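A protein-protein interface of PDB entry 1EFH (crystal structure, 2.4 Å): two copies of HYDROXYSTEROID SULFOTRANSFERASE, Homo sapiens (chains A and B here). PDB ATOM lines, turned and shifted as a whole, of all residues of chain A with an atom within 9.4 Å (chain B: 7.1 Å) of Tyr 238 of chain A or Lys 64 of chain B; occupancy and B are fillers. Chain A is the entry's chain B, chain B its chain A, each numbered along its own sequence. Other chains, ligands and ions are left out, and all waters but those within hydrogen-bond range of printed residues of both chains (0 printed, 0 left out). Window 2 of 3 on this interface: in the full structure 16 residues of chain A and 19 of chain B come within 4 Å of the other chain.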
ATOM      1  N   LYS A 135      11.933   9.316  -1.565  1.00  0.00           N
ATOM      2  CA  LYS A 135      11.359   8.505  -0.495  1.00  0.00           C
ATOM      3  C   LYS A 135       9.848   8.316  -0.561  1.00  0.00           C
ATOM      4  O   LYS A 135       9.366   7.187  -0.581  1.00  0.00           O
ATOM      5  CB  LYS A 135      11.741   9.094   0.866  1.00  0.00           C
ATOM      6  CG  LYS A 135      11.410   8.201   2.038  1.00  0.00           C
ATOM      7  CD  LYS A 135      12.043   8.717   3.317  1.00  0.00           C
ATOM      8  CE  LYS A 135      11.673   7.832   4.488  1.00  0.00           C
ATOM      9  NZ  LYS A 135      10.189   7.750   4.634  1.00  0.00           N
ATOM     10  N   ASN A 136       9.104   9.416  -0.597  1.00  0.00           N
ATOM     11  CA  ASN A 136       7.647   9.344  -0.643  1.00  0.00           C
ATOM     12  C   ASN A 136       7.085   9.356  -2.064  1.00  0.00           C
ATOM     13  O   ASN A 136       6.031   8.773  -2.329  1.00  0.00           O
ATOM     14  CB  ASN A 136       7.051  10.506   0.157  1.00  0.00           C
ATOM     15  CG  ASN A 136       7.423  10.454   1.627  1.00  0.00           C
ATOM     16  OD1 ASN A 136       6.998   9.555   2.359  1.00  0.00           O
ATOM     17  ND2 ASN A 136       8.228  11.419   2.068  1.00  0.00           N
ATOM     18  N   MET A 137       7.803  10.016  -2.969  1.00  0.00           N
ATOM     19  CA  MET A 137       7.406  10.146  -4.370  1.00  0.00           C
ATOM     20  C   MET A 137       6.670   8.956  -4.978  1.00  0.00           C
ATOM     21  O   MET A 137       6.939   7.794  -4.665  1.00  0.00           O
ATOM     22  CB  MET A 137       8.632  10.447  -5.233  1.00  0.00           C
ATOM     23  CG  MET A 137       8.347  11.402  -6.371  1.00  0.00           C
ATOM     24  SD  MET A 137       7.810  12.986  -5.694  1.00  0.00           S
ATOM     25  CE  MET A 137       9.392  13.768  -5.360  1.00  0.00           C
ATOM     26  N   LYS A 138       5.739   9.276  -5.869  1.00  0.00           N
ATOM     27  CA  LYS A 138       4.943   8.278  -6.568  1.00  0.00           C
ATOM     28  C   LYS A 138       5.507   8.137  -7.979  1.00  0.00           C
ATOM     29  O   LYS A 138       6.327   8.952  -8.413  1.00  0.00           O
ATOM     30  CB  LYS A 138       3.478   8.734  -6.642  1.00  0.00           C
ATOM     31  CG  LYS A 138       2.806   8.935  -5.281  1.00  0.00           C
ATOM     32  CD  LYS A 138       1.520   9.765  -5.377  1.00  0.00           C
ATOM     33  CE  LYS A 138       0.457   9.096  -6.242  1.00  0.00           C
ATOM     34  NZ  LYS A 138      -0.807   9.889  -6.297  1.00  0.00           N
ATOM     35  N   TYR A 231       9.243  23.901  -5.891  1.00  0.00           N
ATOM     36  CA  TYR A 231       8.334  22.833  -6.270  1.00  0.00           C
ATOM     37  C   TYR A 231       8.710  22.203  -7.604  1.00  0.00           C
ATOM     38  O   TYR A 231       9.472  22.778  -8.381  1.00  0.00           O
ATOM     39  CB  TYR A 231       6.894  23.347  -6.341  1.00  0.00           C
ATOM     40  CG  TYR A 231       5.902  22.302  -5.898  1.00  0.00           C
ATOM     41  CD1 TYR A 231       5.887  21.856  -4.573  1.00  0.00           C
ATOM     42  CD2 TYR A 231       5.036  21.700  -6.810  1.00  0.00           C
ATOM     43  CE1 TYR A 231       5.043  20.828  -4.164  1.00  0.00           C
ATOM     44  CE2 TYR A 231       4.184  20.666  -6.413  1.00  0.00           C
ATOM     45  CZ  TYR A 231       4.196  20.233  -5.087  1.00  0.00           C
ATOM     46  OH  TYR A 231       3.381  19.194  -4.686  1.00  0.00           O
ATOM     47  N   LEU A 234       6.246  16.554  -9.880  1.00  0.00           N
ATOM     48  CA  LEU A 234       6.388  15.144  -9.538  1.00  0.00           C
ATOM     49  C   LEU A 234       5.461  14.850  -8.362  1.00  0.00           C
ATOM     50  O   LEU A 234       5.803  15.124  -7.210  1.00  0.00           O
ATOM     51  CB  LEU A 234       7.841  14.830  -9.166  1.00  0.00           C
ATOM     52  CG  LEU A 234       8.872  14.879 -10.301  1.00  0.00           C
ATOM     53  CD1 LEU A 234      10.274  14.762  -9.730  1.00  0.00           C
ATOM     54  CD2 LEU A 234       8.603  13.755 -11.293  1.00  0.00           C
ATOM     55  N   SER A 235       4.284  14.307  -8.663  1.00  0.00           N
ATOM     56  CA  SER A 235       3.295  13.982  -7.638  1.00  0.00           C
ATOM     57  C   SER A 235       3.897  13.173  -6.490  1.00  0.00           C
ATOM     58  O   SER A 235       4.540  12.146  -6.708  1.00  0.00           O
ATOM     59  CB  SER A 235       2.125  13.206  -8.254  1.00  0.00           C
ATOM     60  OG  SER A 235       1.393  14.009  -9.160  1.00  0.00           O
ATOM     61  N   VAL A 236       3.674  13.644  -5.266  1.00  0.00           N
ATOM     62  CA  VAL A 236       4.194  12.976  -4.076  1.00  0.00           C
ATOM     63  C   VAL A 236       3.054  12.476  -3.193  1.00  0.00           C
ATOM     64  O   VAL A 236       2.109  13.216  -2.915  1.00  0.00           O
ATOM     65  CB  VAL A 236       5.060  13.935  -3.220  1.00  0.00           C
ATOM     66  CG1 VAL A 236       6.160  13.148  -2.520  1.00  0.00           C
ATOM     67  CG2 VAL A 236       5.631  15.055  -4.083  1.00  0.00           C
ATOM     68  N   ASP A 237       3.144  11.221  -2.759  1.00  0.00           N
ATOM     69  CA  ASP A 237       2.128  10.647  -1.880  1.00  0.00           C
ATOM     70  C   ASP A 237       2.344  11.299  -0.518  1.00  0.00           C
ATOM     71  O   ASP A 237       2.873  10.673   0.402  1.00  0.00           O
ATOM     72  CB  ASP A 237       2.307   9.131  -1.778  1.00  0.00           C
ATOM     73  N   TYR A 238       1.933  12.562  -0.411  1.00  0.00           N
ATOM     74  CA  TYR A 238       2.096  13.360   0.804  1.00  0.00           C
ATOM     75  C   TYR A 238       2.244  12.590   2.117  1.00  0.00           C
ATOM     76  O   TYR A 238       1.518  11.628   2.381  1.00  0.00           O
ATOM     77  CB  TYR A 238       0.945  14.361   0.943  1.00  0.00           C
ATOM     78  CG  TYR A 238       1.234  15.423   1.977  1.00  0.00           C
ATOM     79  CD1 TYR A 238       2.251  16.361   1.773  1.00  0.00           C
ATOM     80  CD2 TYR A 238       0.533  15.462   3.182  1.00  0.00           C
ATOM     81  CE1 TYR A 238       2.565  17.310   2.746  1.00  0.00           C
ATOM     82  CE2 TYR A 238       0.838  16.408   4.163  1.00  0.00           C
ATOM     83  CZ  TYR A 238       1.856  17.326   3.938  1.00  0.00           C
ATOM     84  OH  TYR A 238       2.168  18.252   4.908  1.00  0.00           O
ATOM     85  N   VAL A 239       3.195  13.038   2.938  1.00  0.00           N
ATOM     86  CA  VAL A 239       3.464  12.423   4.233  1.00  0.00           C
ATOM     87  C   VAL A 239       3.490  13.484   5.335  1.00  0.00           C
ATOM     88  O   VAL A 239       4.104  14.543   5.184  1.00  0.00           O
ATOM     89  CB  VAL A 239       4.799  11.676   4.189  1.00  0.00           C
ATOM     90  N   LYS A 242       8.886  17.129   5.069  1.00  0.00           N
ATOM     91  CA  LYS A 242       8.421  15.862   4.515  1.00  0.00           C
ATOM     92  C   LYS A 242       8.481  15.840   2.979  1.00  0.00           C
ATOM     93  O   LYS A 242       7.441  15.812   2.307  1.00  0.00           O
ATOM     94  CB  LYS A 242       6.993  15.575   4.992  1.00  0.00           C
ATOM     95  N   ALA A 243       9.702  15.864   2.441  1.00  0.00           N
ATOM     96  CA  ALA A 243       9.957  15.824   0.996  1.00  0.00           C
ATOM     97  C   ALA A 243       9.783  17.137   0.220  1.00  0.00           C
ATOM     98  O   ALA A 243       9.003  17.204  -0.736  1.00  0.00           O
ATOM     99  CB  ALA A 243       9.112  14.717   0.343  1.00  0.00           C
ATOM    100  N   GLN A 244      10.518  18.173   0.619  1.00  0.00           N
ATOM    101  CA  GLN A 244      10.460  19.460  -0.069  1.00  0.00           C
ATOM    102  C   GLN A 244      11.675  19.557  -0.999  1.00  0.00           C
ATOM    103  O   GLN A 244      12.728  18.989  -0.713  1.00  0.00           O
ATOM    104  CB  GLN A 244      10.463  20.606   0.942  1.00  0.00           C
ATOM    105  N   LEU B  56     -10.495  18.938   1.774  1.00  0.00           N
ATOM    106  CA  LEU B  56     -10.667  19.076   3.215  1.00  0.00           C
ATOM    107  C   LEU B  56     -11.513  17.947   3.788  1.00  0.00           C
ATOM    108  O   LEU B  56     -11.324  17.549   4.934  1.00  0.00           O
ATOM    109  CB  LEU B  56     -11.282  20.439   3.554  1.00  0.00           C
ATOM    110  CG  LEU B  56     -10.282  21.604   3.524  1.00  0.00           C
ATOM    111  CD1 LEU B  56     -10.986  22.949   3.511  1.00  0.00           C
ATOM    112  CD2 LEU B  56      -9.391  21.494   4.740  1.00  0.00           C
ATOM    113  N   SER B  59      -9.110  15.111   4.266  1.00  0.00           N
ATOM    114  CA  SER B  59      -8.232  15.295   5.418  1.00  0.00           C
ATOM    115  C   SER B  59      -9.017  15.534   6.703  1.00  0.00           C
ATOM    116  O   SER B  59      -8.459  15.983   7.700  1.00  0.00           O
ATOM    117  CB  SER B  59      -7.297  16.476   5.181  1.00  0.00           C
ATOM    118  OG  SER B  59      -8.023  17.689   5.150  1.00  0.00           O
ATOM    119  N   GLY B  61     -10.612  17.783   7.739  1.00  0.00           N
ATOM    120  CA  GLY B  61     -10.443  19.101   8.325  1.00  0.00           C
ATOM    121  C   GLY B  61      -9.016  19.593   8.476  1.00  0.00           C
ATOM    122  O   GLY B  61      -8.773  20.802   8.424  1.00  0.00           O
ATOM    123  N   ASP B  62      -8.069  18.679   8.676  1.00  0.00           N
ATOM    124  CA  ASP B  62      -6.668  19.080   8.821  1.00  0.00           C
ATOM    125  C   ASP B  62      -6.241  19.848   7.564  1.00  0.00           C
ATOM    126  O   ASP B  62      -6.573  19.459   6.442  1.00  0.00           O
ATOM    127  CB  ASP B  62      -5.765  17.853   9.033  1.00  0.00           C
ATOM    128  CG  ASP B  62      -4.393  18.229   9.584  1.00  0.00           C
ATOM    129  OD1 ASP B  62      -4.346  18.869  10.660  1.00  0.00           O
ATOM    130  OD2 ASP B  62      -3.366  17.886   8.952  1.00  0.00           O
ATOM    131  N   ALA B  63      -5.503  20.933   7.761  1.00  0.00           N
ATOM    132  CA  ALA B  63      -5.080  21.766   6.650  1.00  0.00           C
ATOM    133  C   ALA B  63      -3.632  21.606   6.197  1.00  0.00           C
ATOM    134  O   ALA B  63      -3.209  22.267   5.247  1.00  0.00           O
ATOM    135  CB  ALA B  63      -5.349  23.230   6.992  1.00  0.00           C
ATOM    136  N   LYS B  64      -2.868  20.741   6.856  1.00  0.00           N
ATOM    137  CA  LYS B  64      -1.466  20.571   6.478  1.00  0.00           C
ATOM    138  C   LYS B  64      -1.273  20.255   5.006  1.00  0.00           C
ATOM    139  O   LYS B  64      -0.492  20.911   4.320  1.00  0.00           O
ATOM    140  CB  LYS B  64      -0.798  19.485   7.324  1.00  0.00           C
ATOM    141  CG  LYS B  64      -0.373  19.959   8.713  1.00  0.00           C
ATOM    142  CD  LYS B  64       0.525  18.921   9.385  1.00  0.00           C
ATOM    143  CE  LYS B  64       0.868  19.317  10.833  1.00  0.00           C
ATOM    144  NZ  LYS B  64       1.860  18.345  11.435  1.00  0.00           N
ATOM    145  N   TRP B  65      -1.999  19.253   4.527  1.00  0.00           N
ATOM    146  CA  TRP B  65      -1.917  18.832   3.135  1.00  0.00           C
ATOM    147  C   TRP B  65      -2.291  19.920   2.116  1.00  0.00           C
ATOM    148  O   TRP B  65      -1.558  20.145   1.152  1.00  0.00           O
ATOM    149  CB  TRP B  65      -2.791  17.586   2.936  1.00  0.00           C
ATOM    150  CG  TRP B  65      -2.849  17.080   1.529  1.00  0.00           C
ATOM    151  CD1 TRP B  65      -1.796  16.871   0.685  1.00  0.00           C
ATOM    152  CD2 TRP B  65      -4.025  16.702   0.807  1.00  0.00           C
ATOM    153  NE1 TRP B  65      -2.243  16.387  -0.521  1.00  0.00           N
ATOM    154  CE2 TRP B  65      -3.607  16.273  -0.476  1.00  0.00           C
ATOM    155  CE3 TRP B  65      -5.393  16.683   1.116  1.00  0.00           C
ATOM    156  CZ2 TRP B  65      -4.507  15.830  -1.449  1.00  0.00           C
ATOM    157  CZ3 TRP B  65      -6.288  16.240   0.146  1.00  0.00           C
ATOM    158  CH2 TRP B  65      -5.838  15.820  -1.122  1.00  0.00           C
ATOM    159  N   ILE B  66      -3.416  20.602   2.322  1.00  0.00           N
ATOM    160  CA  ILE B  66      -3.834  21.639   1.379  1.00  0.00           C
ATOM    161  C   ILE B  66      -2.952  22.872   1.408  1.00  0.00           C
ATOM    162  O   ILE B  66      -3.026  23.708   0.517  1.00  0.00           O
ATOM    163  CB  ILE B  66      -5.287  22.099   1.623  1.00  0.00           C
ATOM    164  CG1 ILE B  66      -5.433  22.661   3.040  1.00  0.00           C
ATOM    165  CG2 ILE B  66      -6.241  20.940   1.390  1.00  0.00           C
ATOM    166  CD1 ILE B  66      -6.800  23.289   3.312  1.00  0.00           C
ATOM    167  N   GLN B  67      -2.109  22.983   2.427  1.00  0.00           N
ATOM    168  CA  GLN B  67      -1.240  24.142   2.538  1.00  0.00           C
ATOM    169  C   GLN B  67       0.188  23.877   2.090  1.00  0.00           C
ATOM    170  O   GLN B  67       1.003  24.795   2.024  1.00  0.00           O
ATOM    171  CB  GLN B  67      -1.262  24.657   3.973  1.00  0.00           C
ATOM    172  CG  GLN B  67      -2.655  25.040   4.417  1.00  0.00           C
ATOM    173  CD  GLN B  67      -2.674  25.775   5.734  1.00  0.00           C
ATOM    174  OE1 GLN B  67      -2.256  25.240   6.765  1.00  0.00           O
ATOM    175  NE2 GLN B  67      -3.162  27.012   5.713  1.00  0.00           N
ATOM    176  N   SER B  68       0.490  22.624   1.769  1.00  0.00           N
ATOM    177  CA  SER B  68       1.832  22.268   1.317  1.00  0.00           C
ATOM    178  C   SER B  68       1.851  21.819  -0.145  1.00  0.00           C
ATOM    179  O   SER B  68       2.872  21.932  -0.821  1.00  0.00           O
ATOM    180  CB  SER B  68       2.431  21.181   2.226  1.00  0.00           C
ATOM    181  OG  SER B  68       1.554  20.080   2.385  1.00  0.00           O
ATOM    182  N   VAL B  69       0.717  21.317  -0.628  1.00  0.00           N
ATOM    183  CA  VAL B  69       0.585  20.859  -2.016  1.00  0.00           C
ATOM    184  C   VAL B  69      -0.394  21.788  -2.741  1.00  0.00           C
ATOM    185  O   VAL B  69      -1.515  21.998  -2.280  1.00  0.00           O
ATOM    186  CB  VAL B  69       0.054  19.400  -2.074  1.00  0.00           C
ATOM    187  CG1 VAL B  69      -0.207  18.993  -3.513  1.00  0.00           C
ATOM    188  CG2 VAL B  69       1.063  18.453  -1.430  1.00  0.00           C
ATOM    189  N   ASN B 217     -11.571  26.272   7.230  1.00  0.00           N
ATOM    190  CA  ASN B 217     -10.497  26.229   6.245  1.00  0.00           C
ATOM    191  C   ASN B 217     -10.897  26.378   4.780  1.00  0.00           C
ATOM    192  O   ASN B 217     -10.029  26.497   3.923  1.00  0.00           O
ATOM    193  CB  ASN B 217      -9.677  24.942   6.423  1.00  0.00           C
ATOM    194  CG  ASN B 217      -8.798  24.971   7.667  1.00  0.00           C
ATOM    195  OD1 ASN B 217      -8.020  25.904   7.867  1.00  0.00           O
ATOM    196  ND2 ASN B 217      -8.912  23.947   8.501  1.00  0.00           N
ATOM    197  N   ASN B 226      -4.187  31.192   1.556  1.00  0.00           N
ATOM    198  CA  ASN B 226      -3.443  29.955   1.335  1.00  0.00           C
ATOM    199  C   ASN B 226      -2.770  29.955  -0.037  1.00  0.00           C
ATOM    200  O   ASN B 226      -3.419  29.732  -1.061  1.00  0.00           O
ATOM    201  CB  ASN B 226      -4.362  28.736   1.441  1.00  0.00           C
ATOM    202  CG  ASN B 226      -3.589  27.424   1.409  1.00  0.00           C
ATOM    203  OD1 ASN B 226      -2.454  27.372   0.942  1.00  0.00           O
ATOM    204  ND2 ASN B 226      -4.211  26.356   1.894  1.00  0.00           N
ATOM    205  N   MET B 228      -1.092  27.835  -1.540  1.00  0.00           N
ATOM    206  CA  MET B 228      -1.289  26.593  -2.283  1.00  0.00           C
ATOM    207  C   MET B 228      -2.647  26.481  -2.982  1.00  0.00           C
ATOM    208  O   MET B 228      -2.773  25.795  -4.003  1.00  0.00           O
ATOM    209  CB  MET B 228      -1.115  25.388  -1.352  1.00  0.00           C
ATOM    210  CG  MET B 228       0.293  25.199  -0.813  1.00  0.00           C
ATOM    211  SD  MET B 228       1.528  24.947  -2.108  1.00  0.00           S
ATOM    212  CE  MET B 228       2.064  26.632  -2.377  1.00  0.00           C
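No position is printed for both chains.
The side-chain hydroxyl (OG) of Ser 68 of chain B sits close to the side-chain hydroxyl (OH) of Tyr 238 of chain A (3.2 Å).
O of Lys 64 of chain B lies within hydrogen-bond range of OG of Ser 68 of chain B (2.9 Å). OG of Ser 68 of chain B sits at hydrogen-bond distance from O of Trp 65 of chain B (3.3 Å).
Of the printed residues of chain A, Lys 64 of chain B touches Tyr 238. Of the printed residues of chain A, Val 69 of chain B touches Tyr 231. Of the printed residues of chain A, Trp 65 of chain B touches Tyr 238. The nearest printed residue of chain B that does not touch Tyr 238 of chain A is Val 69 of chain B (4.01 Å). The nearest residue of chain A that does not touch Lys 64 of chain B is Val 239 of chain A (7.0 Å).
Tyr 231 of chain A touches Val 69 of chain B. O of Lys 64 of chain B touches OH of Tyr 238 of chain A, at 3.8 Å. Tyr 238 of chain A touches Trp 65 of chain B.
Of the 14 printed residues of chain B, 4 touch a printed residue of chain A. Printed residues of chain B that touch a printed residue of chain A: Lys 64, Trp 65, Ser 68 and Val 69. Hydrophobic or aromatic side chains of chain B within 4 Å of the printed part of chain A: Trp 65 and Val 69. Along chain B the printed residues that touch a printed residue of chain A span positions 64 to 69.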
